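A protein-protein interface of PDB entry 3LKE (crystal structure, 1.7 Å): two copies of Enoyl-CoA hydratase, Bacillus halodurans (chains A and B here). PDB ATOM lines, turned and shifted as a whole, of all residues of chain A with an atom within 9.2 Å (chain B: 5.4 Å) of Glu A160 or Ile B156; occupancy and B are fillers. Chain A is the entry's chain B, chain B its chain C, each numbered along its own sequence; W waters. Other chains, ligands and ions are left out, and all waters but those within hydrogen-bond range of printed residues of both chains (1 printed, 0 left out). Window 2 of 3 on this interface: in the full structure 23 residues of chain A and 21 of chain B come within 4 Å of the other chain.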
ATOM      1  N   LEU A 153      -1.647  12.810  27.872  1.00  0.00           N
ATOM      2  CA  LEU A 153      -2.403  12.801  26.613  1.00  0.00           C
ATOM      3  C   LEU A 153      -3.697  11.972  26.695  1.00  0.00           C
ATOM      4  O   LEU A 153      -4.770  12.463  26.377  1.00  0.00           O
ATOM      5  CB  LEU A 153      -1.536  12.384  25.414  1.00  0.00           C
ATOM      6  CG  LEU A 153      -0.391  13.360  25.065  1.00  0.00           C
ATOM      7  CD1 LEU A 153       0.509  12.808  23.954  1.00  0.00           C
ATOM      8  CD2 LEU A 153      -0.971  14.713  24.645  1.00  0.00           C
ATOM      9  N   PRO A 154      -3.607  10.710  27.132  1.00  0.00           N
ATOM     10  CA  PRO A 154      -4.857   9.940  27.118  1.00  0.00           C
ATOM     11  C   PRO A 154      -5.911  10.489  28.089  1.00  0.00           C
ATOM     12  O   PRO A 154      -7.130  10.378  27.866  1.00  0.00           O
ATOM     13  CB  PRO A 154      -4.425   8.533  27.546  1.00  0.00           C
ATOM     14  CG  PRO A 154      -3.049   8.676  28.133  1.00  0.00           C
ATOM     15  CD  PRO A 154      -2.441   9.918  27.558  1.00  0.00           C
ATOM     16  N   ARG A 155      -5.456  11.076  29.181  1.00  0.00           N
ATOM     17  CA  ARG A 155      -6.397  11.598  30.160  1.00  0.00           C
ATOM     18  C   ARG A 155      -7.062  12.876  29.687  1.00  0.00           C
ATOM     19  O   ARG A 155      -8.180  13.175  30.093  1.00  0.00           O
ATOM     20  CB  ARG A 155      -5.724  11.789  31.509  1.00  0.00           C
ATOM     21  CG  ARG A 155      -5.463  10.456  32.190  1.00  0.00           C
ATOM     22  CD  ARG A 155      -4.585  10.572  33.436  1.00  0.00           C
ATOM     23  NE  ARG A 155      -4.448   9.273  34.097  1.00  0.00           N
ATOM     24  CZ  ARG A 155      -3.719   8.265  33.617  1.00  0.00           C
ATOM     25  NH1 ARG A 155      -3.071   8.388  32.462  1.00  0.00           N
ATOM     26  NH2 ARG A 155      -3.652   7.121  34.287  1.00  0.00           N
ATOM     27  N   ILE A 157      -7.199  13.981  26.084  1.00  0.00           N
ATOM     28  CA  ILE A 157      -7.828  13.871  24.764  1.00  0.00           C
ATOM     29  C   ILE A 157      -8.375  12.470  24.463  1.00  0.00           C
ATOM     30  O   ILE A 157      -9.035  12.254  23.437  1.00  0.00           O
ATOM     31  CB  ILE A 157      -6.869  14.328  23.630  1.00  0.00           C
ATOM     32  CG1 ILE A 157      -5.826  13.244  23.316  1.00  0.00           C
ATOM     33  CG2 ILE A 157      -6.189  15.651  24.000  1.00  0.00           C
ATOM     34  CD1 ILE A 157      -4.979  13.529  22.066  1.00  0.00           C
ATOM     35  N   GLY A 158      -8.102  11.523  25.359  1.00  0.00           N
ATOM     36  CA  GLY A 158      -8.599  10.160  25.219  1.00  0.00           C
ATOM     37  C   GLY A 158      -7.564   9.248  24.566  1.00  0.00           C
ATOM     38  O   GLY A 158      -6.737   9.700  23.803  1.00  0.00           O
ATOM     39  N   TYR A 159      -7.636   7.952  24.854  1.00  0.00           N
ATOM     40  CA  TYR A 159      -6.640   7.019  24.322  1.00  0.00           C
ATOM     41  C   TYR A 159      -6.659   6.933  22.799  1.00  0.00           C
ATOM     42  O   TYR A 159      -5.613   6.957  22.162  1.00  0.00           O
ATOM     43  CB  TYR A 159      -6.845   5.626  24.903  1.00  0.00           C
ATOM     44  CG  TYR A 159      -5.951   4.577  24.291  1.00  0.00           C
ATOM     45  CD1 TYR A 159      -4.661   4.368  24.768  1.00  0.00           C
ATOM     46  CD2 TYR A 159      -6.399   3.796  23.230  1.00  0.00           C
ATOM     47  CE1 TYR A 159      -3.841   3.406  24.207  1.00  0.00           C
ATOM     48  CE2 TYR A 159      -5.602   2.831  22.678  1.00  0.00           C
ATOM     49  CZ  TYR A 159      -4.316   2.651  23.153  1.00  0.00           C
ATOM     50  OH  TYR A 159      -3.520   1.695  22.587  1.00  0.00           O
ATOM     51  N   GLU A 160      -7.847   6.793  22.220  1.00  0.00           N
ATOM     52  CA  GLU A 160      -7.925   6.600  20.784  1.00  0.00           C
ATOM     53  C   GLU A 160      -7.393   7.832  20.063  1.00  0.00           C
ATOM     54  O   GLU A 160      -6.699   7.710  19.059  1.00  0.00           O
ATOM     55  CB  GLU A 160      -9.365   6.297  20.349  1.00  0.00           C
ATOM     56  CG  GLU A 160      -9.896   4.972  20.855  1.00  0.00           C
ATOM     57  CD  GLU A 160     -10.560   5.062  22.233  1.00  0.00           C
ATOM     58  OE1 GLU A 160     -10.356   6.055  22.978  1.00  0.00           O
ATOM     59  OE2 GLU A 160     -11.308   4.119  22.563  1.00  0.00           O
ATOM     60  N   GLN A 161      -7.714   9.017  20.570  1.00  0.00           N
ATOM     61  CA  GLN A 161      -7.265  10.242  19.905  1.00  0.00           C
ATOM     62  C   GLN A 161      -5.773  10.426  20.128  1.00  0.00           C
ATOM     63  O   GLN A 161      -5.085  11.036  19.313  1.00  0.00           O
ATOM     64  CB  GLN A 161      -8.032  11.463  20.419  1.00  0.00           C
ATOM     65  CG  GLN A 161      -9.451  11.558  19.854  1.00  0.00           C
ATOM     66  CD  GLN A 161     -10.105  12.906  20.123  1.00  0.00           C
ATOM     67  OE1 GLN A 161     -10.060  13.426  21.243  1.00  0.00           O
ATOM     68  NE2 GLN A 161     -10.734  13.473  19.091  1.00  0.00           N
ATOM     69  N   THR A 162      -5.266   9.897  21.235  1.00  0.00           N
ATOM     70  CA  THR A 162      -3.819   9.947  21.475  1.00  0.00           C
ATOM     71  C   THR A 162      -3.077   9.075  20.478  1.00  0.00           C
ATOM     72  O   THR A 162      -2.068   9.486  19.907  1.00  0.00           O
ATOM     73  CB  THR A 162      -3.465   9.493  22.896  1.00  0.00           C
ATOM     74  OG1 THR A 162      -3.988  10.442  23.827  1.00  0.00           O
ATOM     75  CG2 THR A 162      -1.956   9.419  23.103  1.00  0.00           C
ATOM     76  N   MET A 163      -3.567   7.860  20.268  1.00  0.00           N
ATOM     77  CA  MET A 163      -2.921   6.996  19.296  1.00  0.00           C
ATOM     78  C   MET A 163      -2.925   7.664  17.917  1.00  0.00           C
ATOM     79  O   MET A 163      -1.928   7.618  17.186  1.00  0.00           O
ATOM     80  CB  MET A 163      -3.581   5.618  19.243  1.00  0.00           C
ATOM     81  CG  MET A 163      -3.189   4.708  20.419  1.00  0.00           C
ATOM     82  SD  MET A 163      -1.442   4.242  20.566  1.00  0.00           S
ATOM     83  CE  MET A 163      -1.339   3.111  19.166  1.00  0.00           C
ATOM     84  N   ASN A 164      -4.040   8.307  17.574  1.00  0.00           N
ATOM     85  CA  ASN A 164      -4.140   8.912  16.246  1.00  0.00           C
ATOM     86  C   ASN A 164      -3.267  10.156  16.092  1.00  0.00           C
ATOM     87  O   ASN A 164      -2.653  10.368  15.044  1.00  0.00           O
ATOM     88  CB  ASN A 164      -5.585   9.255  15.899  1.00  0.00           C
ATOM     89  CG  ASN A 164      -5.801   9.314  14.404  1.00  0.00           C
ATOM     90  OD1 ASN A 164      -6.280  10.313  13.868  1.00  0.00           O
ATOM     91  ND2 ASN A 164      -5.415   8.253  13.723  1.00  0.00           N
ATOM     92  N   LEU A 165      -3.241  10.986  17.129  1.00  0.00           N
ATOM     93  CA  LEU A 165      -2.355  12.155  17.151  1.00  0.00           C
ATOM     94  C   LEU A 165      -0.890  11.757  16.970  1.00  0.00           C
ATOM     95  O   LEU A 165      -0.141  12.403  16.232  1.00  0.00           O
ATOM     96  CB  LEU A 165      -2.520  12.906  18.472  1.00  0.00           C
ATOM     97  CG  LEU A 165      -1.730  14.206  18.627  1.00  0.00           C
ATOM     98  CD1 LEU A 165      -2.272  15.249  17.681  1.00  0.00           C
ATOM     99  CD2 LEU A 165      -1.819  14.693  20.059  1.00  0.00           C
ATOM    100  N   LEU A 166      -0.472  10.709  17.663  1.00  0.00           N
ATOM    101  CA  LEU A 166       0.915  10.277  17.592  1.00  0.00           C
ATOM    102  C   LEU A 166       1.202   9.672  16.227  1.00  0.00           C
ATOM    103  O   LEU A 166       2.273   9.888  15.652  1.00  0.00           O
ATOM    104  CB  LEU A 166       1.219   9.272  18.708  1.00  0.00           C
ATOM    105  CG  LEU A 166       1.113   9.838  20.124  1.00  0.00           C
ATOM    106  CD1 LEU A 166       1.258   8.723  21.155  1.00  0.00           C
ATOM    107  CD2 LEU A 166       2.150  10.933  20.351  1.00  0.00           C
ATOM    108  N   LEU A 167       0.239   8.930  15.696  1.00  0.00           N
ATOM    109  CA  LEU A 167       0.441   8.266  14.411  1.00  0.00           C
ATOM    110  C   LEU A 167       0.623   9.297  13.306  1.00  0.00           C
ATOM    111  O   LEU A 167       1.518   9.162  12.450  1.00  0.00           O
ATOM    112  CB  LEU A 167      -0.765   7.389  14.086  1.00  0.00           C
ATOM    113  CG  LEU A 167      -0.619   6.195  13.143  1.00  0.00           C
ATOM    114  CD1 LEU A 167      -1.765   6.156  12.129  1.00  0.00           C
ATOM    115  CD2 LEU A 167       0.732   6.162  12.454  1.00  0.00           C
ATOM    116  N   GLU A 168      -0.215  10.325  13.314  1.00  0.00           N
ATOM    117  CA  GLU A 168      -0.184  11.340  12.254  1.00  0.00           C
ATOM    118  C   GLU A 168       1.058  12.244  12.313  1.00  0.00           C
ATOM    119  O   GLU A 168       1.627  12.616  11.274  1.00  0.00           O
ATOM    120  CB  GLU A 168      -1.484  12.143  12.246  1.00  0.00           C
ATOM    121  CG  GLU A 168      -2.668  11.279  11.830  1.00  0.00           C
ATOM    122  CD  GLU A 168      -3.943  12.052  11.563  1.00  0.00           C
ATOM    123  OE1 GLU A 168      -3.990  13.263  11.879  1.00  0.00           O
ATOM    124  OE2 GLU A 168      -4.912  11.431  11.048  1.00  0.00           O
ATOM    125  N   LEU A 180      -9.133  19.662  20.776  1.00  0.00           N
ATOM    126  CA  LEU A 180      -8.749  18.451  21.472  1.00  0.00           C
ATOM    127  C   LEU A 180      -8.778  18.628  22.984  1.00  0.00           C
ATOM    128  O   LEU A 180      -8.933  17.653  23.721  1.00  0.00           O
ATOM    129  CB  LEU A 180      -7.353  18.013  21.027  1.00  0.00           C
ATOM    130  CG  LEU A 180      -7.275  17.488  19.597  1.00  0.00           C
ATOM    131  CD1 LEU A 180      -5.830  17.275  19.215  1.00  0.00           C
ATOM    132  CD2 LEU A 180      -8.066  16.201  19.479  1.00  0.00           C
ATOM    133  N   LEU B 121     -14.217  -2.770  20.845  1.00  0.00           N
ATOM    134  CA  LEU B 121     -13.888  -1.581  21.626  1.00  0.00           C
ATOM    135  C   LEU B 121     -12.489  -1.665  22.247  1.00  0.00           C
ATOM    136  O   LEU B 121     -11.949  -0.658  22.707  1.00  0.00           O
ATOM    137  CB  LEU B 121     -14.934  -1.323  22.711  1.00  0.00           C
ATOM    138  CG  LEU B 121     -16.310  -0.927  22.174  1.00  0.00           C
ATOM    139  CD1 LEU B 121     -17.293  -0.827  23.345  1.00  0.00           C
ATOM    140  CD2 LEU B 121     -16.182   0.397  21.424  1.00  0.00           C
ATOM    141  N   CYS B 123      -9.912  -2.312  20.463  1.00  0.00           N
ATOM    142  CA  CYS B 123      -8.985  -1.898  19.411  1.00  0.00           C
ATOM    143  C   CYS B 123      -8.570  -0.456  19.588  1.00  0.00           C
ATOM    144  O   CYS B 123      -9.299   0.341  20.213  1.00  0.00           O
ATOM    145  CB  CYS B 123      -9.621  -2.050  18.032  1.00  0.00           C
ATOM    146  SG  CYS B 123      -9.908  -3.760  17.519  1.00  0.00           S
ATOM    147  N   ASP B 124      -7.399  -0.136  19.040  1.00  0.00           N
ATOM    148  CA  ASP B 124      -6.892   1.233  19.023  1.00  0.00           C
ATOM    149  C   ASP B 124      -7.753   2.176  18.184  1.00  0.00           C
ATOM    150  O   ASP B 124      -7.838   3.374  18.467  1.00  0.00           O
ATOM    151  CB  ASP B 124      -5.467   1.283  18.481  1.00  0.00           C
ATOM    152  CG  ASP B 124      -4.481   0.519  19.330  1.00  0.00           C
ATOM    153  OD1 ASP B 124      -4.652   0.466  20.564  1.00  0.00           O
ATOM    154  OD2 ASP B 124      -3.492   0.000  18.757  1.00  0.00           O
ATOM    155  N   ARG B 125      -8.372   1.641  17.137  1.00  0.00           N
ATOM    156  CA  ARG B 125      -9.186   2.471  16.271  1.00  0.00           C
ATOM    157  C   ARG B 125     -10.307   1.630  15.696  1.00  0.00           C
ATOM    158  O   ARG B 125     -10.083   0.499  15.280  1.00  0.00           O
ATOM    159  CB  ARG B 125      -8.345   3.073  15.137  1.00  0.00           C
ATOM    160  CG  ARG B 125      -9.028   4.233  14.405  1.00  0.00           C
ATOM    161  CD  ARG B 125      -8.034   5.048  13.573  1.00  0.00           C
ATOM    162  NE  ARG B 125      -8.653   6.276  13.070  1.00  0.00           N
ATOM    163  CZ  ARG B 125      -8.824   7.377  13.795  1.00  0.00           C
ATOM    164  NH1 ARG B 125      -8.432   7.406  15.062  1.00  0.00           N
ATOM    165  NH2 ARG B 125      -9.395   8.450  13.260  1.00  0.00           N
ATOM    166  N   ARG B 126     -11.503   2.201  15.685  1.00  0.00           N
ATOM    167  CA  ARG B 126     -12.666   1.559  15.087  1.00  0.00           C
ATOM    168  C   ARG B 126     -13.139   2.475  13.970  1.00  0.00           C
ATOM    169  O   ARG B 126     -13.449   3.642  14.201  1.00  0.00           O
ATOM    170  CB  ARG B 126     -13.785   1.329  16.113  1.00  0.00           C
ATOM    171  CG  ARG B 126     -13.530   0.196  17.126  1.00  0.00           C
ATOM    172  CD  ARG B 126     -12.733   0.670  18.345  1.00  0.00           C
ATOM    173  NE  ARG B 126     -13.443   1.713  19.088  1.00  0.00           N
ATOM    174  CZ  ARG B 126     -12.941   2.352  20.142  1.00  0.00           C
ATOM    175  NH1 ARG B 126     -11.726   2.061  20.591  1.00  0.00           N
ATOM    176  NH2 ARG B 126     -13.641   3.300  20.735  1.00  0.00           N
ATOM    177  N   PHE B 152     -15.402  -0.974  28.940  1.00  0.00           N
ATOM    178  CA  PHE B 152     -15.191  -0.035  27.839  1.00  0.00           C
ATOM    179  C   PHE B 152     -16.243   1.063  27.706  1.00  0.00           C
ATOM    180  O   PHE B 152     -15.899   2.217  27.484  1.00  0.00           O
ATOM    181  CB  PHE B 152     -15.029  -0.773  26.523  1.00  0.00           C
ATOM    182  CG  PHE B 152     -13.721  -1.509  26.417  1.00  0.00           C
ATOM    183  CD1 PHE B 152     -12.532  -0.802  26.376  1.00  0.00           C
ATOM    184  CD2 PHE B 152     -13.684  -2.894  26.384  1.00  0.00           C
ATOM    185  CE1 PHE B 152     -11.325  -1.470  26.284  1.00  0.00           C
ATOM    186  CE2 PHE B 152     -12.469  -3.570  26.288  1.00  0.00           C
ATOM    187  CZ  PHE B 152     -11.296  -2.851  26.242  1.00  0.00           C
ATOM    188  N   LEU B 153     -17.519   0.722  27.828  1.00  0.00           N
ATOM    189  CA  LEU B 153     -18.545   1.741  27.604  1.00  0.00           C
ATOM    190  C   LEU B 153     -18.412   2.998  28.500  1.00  0.00           C
ATOM    191  O   LEU B 153     -18.393   4.119  27.987  1.00  0.00           O
ATOM    192  CB  LEU B 153     -19.959   1.146  27.665  1.00  0.00           C
ATOM    193  CG  LEU B 153     -20.332   0.182  26.529  1.00  0.00           C
ATOM    194  CD1 LEU B 153     -21.668  -0.489  26.835  1.00  0.00           C
ATOM    195  CD2 LEU B 153     -20.374   0.849  25.145  1.00  0.00           C
ATOM    196  N   PRO B 154     -18.315   2.828  29.824  1.00  0.00           N
ATOM    197  CA  PRO B 154     -18.246   4.059  30.623  1.00  0.00           C
ATOM    198  C   PRO B 154     -16.975   4.863  30.372  1.00  0.00           C
ATOM    199  O   PRO B 154     -16.979   6.093  30.463  1.00  0.00           O
ATOM    200  CB  PRO B 154     -18.266   3.558  32.072  1.00  0.00           C
ATOM    201  CG  PRO B 154     -18.029   2.068  31.991  1.00  0.00           C
ATOM    202  CD  PRO B 154     -18.484   1.622  30.655  1.00  0.00           C
ATOM    203  N   ARG B 155     -15.886   4.169  30.064  1.00  0.00           N
ATOM    204  CA  ARG B 155     -14.624   4.853  29.825  1.00  0.00           C
ATOM    205  C   ARG B 155     -14.629   5.619  28.515  1.00  0.00           C
ATOM    206  O   ARG B 155     -13.962   6.642  28.396  1.00  0.00           O
ATOM    207  CB  ARG B 155     -13.452   3.876  29.898  1.00  0.00           C
ATOM    208  CG  ARG B 155     -13.104   3.563  31.360  1.00  0.00           C
ATOM    209  CD  ARG B 155     -12.060   2.467  31.500  1.00  0.00           C
ATOM    210  NE  ARG B 155     -11.782   2.224  32.916  1.00  0.00           N
ATOM    211  CZ  ARG B 155     -12.584   1.559  33.739  1.00  0.00           C
ATOM    212  NH1 ARG B 155     -13.746   1.080  33.311  1.00  0.00           N
ATOM    213  NH2 ARG B 155     -12.231   1.397  35.013  1.00  0.00           N
ATOM    214  N   ILE B 156     -15.382   5.124  27.540  1.00  0.00           N
ATOM    215  CA  ILE B 156     -15.409   5.753  26.225  1.00  0.00           C
ATOM    216  C   ILE B 156     -16.485   6.837  26.121  1.00  0.00           C
ATOM    217  O   ILE B 156     -16.211   7.948  25.644  1.00  0.00           O
ATOM    218  CB  ILE B 156     -15.627   4.702  25.115  1.00  0.00           C
ATOM    219  CG1 ILE B 156     -14.459   3.715  25.106  1.00  0.00           C
ATOM    220  CG2 ILE B 156     -15.804   5.381  23.750  1.00  0.00           C
ATOM    221  CD1 ILE B 156     -14.571   2.614  24.071  1.00  0.00           C
ATOM    222  N   ILE B 157     -17.697   6.519  26.555  1.00  0.00           N
ATOM    223  CA  ILE B 157     -18.826   7.441  26.365  1.00  0.00           C
ATOM    224  C   ILE B 157     -19.337   8.095  27.631  1.00  0.00           C
ATOM    225  O   ILE B 157     -20.172   8.998  27.563  1.00  0.00           O
ATOM    226  CB  ILE B 157     -19.995   6.784  25.609  1.00  0.00           C
ATOM    227  CG1 ILE B 157     -20.778   5.829  26.517  1.00  0.00           C
ATOM    228  CG2 ILE B 157     -19.483   6.053  24.402  1.00  0.00           C
ATOM    229  CD1 ILE B 157     -22.081   5.336  25.874  1.00  0.00           C
ATOM    230  N   GLY B 158     -18.843   7.643  28.779  1.00  0.00           N
ATOM    231  CA  GLY B 158     -19.276   8.174  30.060  1.00  0.00           C
ATOM    232  C   GLY B 158     -20.279   7.273  30.759  1.00  0.00           C
ATOM    233  O   GLY B 158     -21.028   6.532  30.123  1.00  0.00           O
ATOM    234  N   LEU B 180     -20.608   9.635  19.883  1.00  0.00           N
ATOM    235  CA  LEU B 180     -20.338   9.099  21.216  1.00  0.00           C
ATOM    236  C   LEU B 180     -18.872   8.764  21.463  1.00  0.00           C
ATOM    237  O   LEU B 180     -18.431   8.727  22.619  1.00  0.00           O
ATOM    238  CB  LEU B 180     -21.160   7.841  21.444  1.00  0.00           C
ATOM    239  CG  LEU B 180     -22.655   8.096  21.642  1.00  0.00           C
ATOM    240  CD1 LEU B 180     -23.412   6.806  21.514  1.00  0.00           C
ATOM    241  CD2 LEU B 180     -22.921   8.769  22.991  1.00  0.00           C
ATOM    242  N   GLY B 181     -18.143   8.492  20.389  1.00  0.00           N
ATOM    243  CA  GLY B 181     -16.741   8.117  20.481  1.00  0.00           C
ATOM    244  C   GLY B 181     -16.542   6.610  20.422  1.00  0.00           C
ATOM    245  O   GLY B 181     -15.424   6.113  20.568  1.00  0.00           O
ATOM    246  N   LEU B 182     -17.631   5.877  20.215  1.00  0.00           N
ATOM    247  CA  LEU B 182     -17.537   4.429  20.046  1.00  0.00           C
ATOM    248  C   LEU B 182     -16.736   4.058  18.796  1.00  0.00           C
ATOM    249  O   LEU B 182     -15.962   3.094  18.820  1.00  0.00           O
ATOM    250  CB  LEU B 182     -18.924   3.782  20.054  1.00  0.00           C
ATOM    251  CG  LEU B 182     -19.727   3.904  21.354  1.00  0.00           C
ATOM    252  CD1 LEU B 182     -21.142   3.486  21.085  1.00  0.00           C
ATOM    253  CD2 LEU B 182     -19.102   3.013  22.431  1.00  0.00           C
ATOM    254  N   GLN B 184     -14.136   5.995  15.666  1.00  0.00           N
ATOM    255  CA  GLN B 184     -13.276   7.158  15.496  1.00  0.00           C
ATOM    256  C   GLN B 184     -13.499   7.891  14.183  1.00  0.00           C
ATOM    257  O   GLN B 184     -13.187   9.082  14.062  1.00  0.00           O
ATOM    258  CB  GLN B 184     -11.818   6.717  15.568  1.00  0.00           C
ATOM    259  CG  GLN B 184     -11.318   6.529  17.001  1.00  0.00           C
ATOM    260  CD  GLN B 184     -12.144   5.517  17.797  1.00  0.00           C
ATOM    261  OE1 GLN B 184     -12.134   4.326  17.506  1.00  0.00           O
ATOM    262  NE2 GLN B 184     -12.844   5.995  18.811  1.00  0.00           N
HETATM  263  O   HOH W   1      -7.315   5.768  17.164  1.00  0.00           O
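ND2 of Asn A164 sits close to NH1 of Arg B125 (3.4 Å).
The side-chain hydroxyl (OH) of Tyr A159 lies within hydrogen-bond range of the side-chain carboxylate (OD1) of Asp B124 (2.6 Å).
The side-chain carboxylate of Glu A160 is in salt-bridge range of the guanidinium group of Arg B126 (2.9 Å).
The guanidinium group (NH1) of Arg B126 is in hydrogen-bond range of the backbone carbonyl oxygen (O) of Leu B121, at 3.5 Å.
The guanidinium group of Arg B126 is in hydrogen-bond range of the backbone carbonyl oxygen of Leu B182, at 2.9 Å.
The guanidinium group (NH1) of Arg B126 sits at hydrogen-bond distance from the backbone carbonyl oxygen (O) of Cys B123 (3.0 Å).
The backbone carbonyl oxygen (O) of Arg B126 sits at hydrogen-bond distance from the backbone NH (N) of Gln B184, at 2.9 Å.
NE2 of Gln B184 sits at hydrogen-bond distance from O of Gly B181, 3.1 Å away.
The side-chain carboxylate (OE2) of Glu A168 sits close to the side-chain amide oxygen (OD1) of Asn A164 (3.3 Å).
Glu A160 touches Asp B124.
Glu A160 touches Ile B156.
CG of Glu A160 touches NE2 of Gln B184, 3.7 Å away.
Met A163 touches Asp B124 (CE to OD2, 3.8 Å).
Glu A160 touches just these residues of chain B: Asp B124, Arg B126, Ile B156 and Gln B184.
No residue of chain A comes within 4 Å of Gly B181.
Of the printed residues of chain B, Asn A164 touches Arg B125 (3.3 Å).
Of the printed residues of chain A, Gln B184 touches Glu A160 (3.7 Å).
Thr A162 touches none of the printed residues of chain B.
Leu A165 touches none of the printed residues of chain B.
The nearest residue of chain B that does not touch Glu A160 is Arg B125 (4.4 Å).
Of the 16 printed residues of chain B, 5 touch a printed residue of chain A.
Hydrophobic or aromatic side chains of chain B within 4 Å of the printed part of chain A: Ile B156.
Of the 16 printed residues of chain A, 4 touch a printed residue of chain B.
Positions printed for both chains: 153, 154, 155, 157, 158 and 180.
Of the 7 pairs that touch across the chains among the printed residues, none has its exchanged pair printed and touching as well.
Water W1 lies within hydrogen-bond range of the backbone carbonyl oxygen of Asp B124 (2.8 Å), the backbone carbonyl oxygen of Glu A160 (2.8 Å) and the guanidinium group of Arg B125 (2.9 Å).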
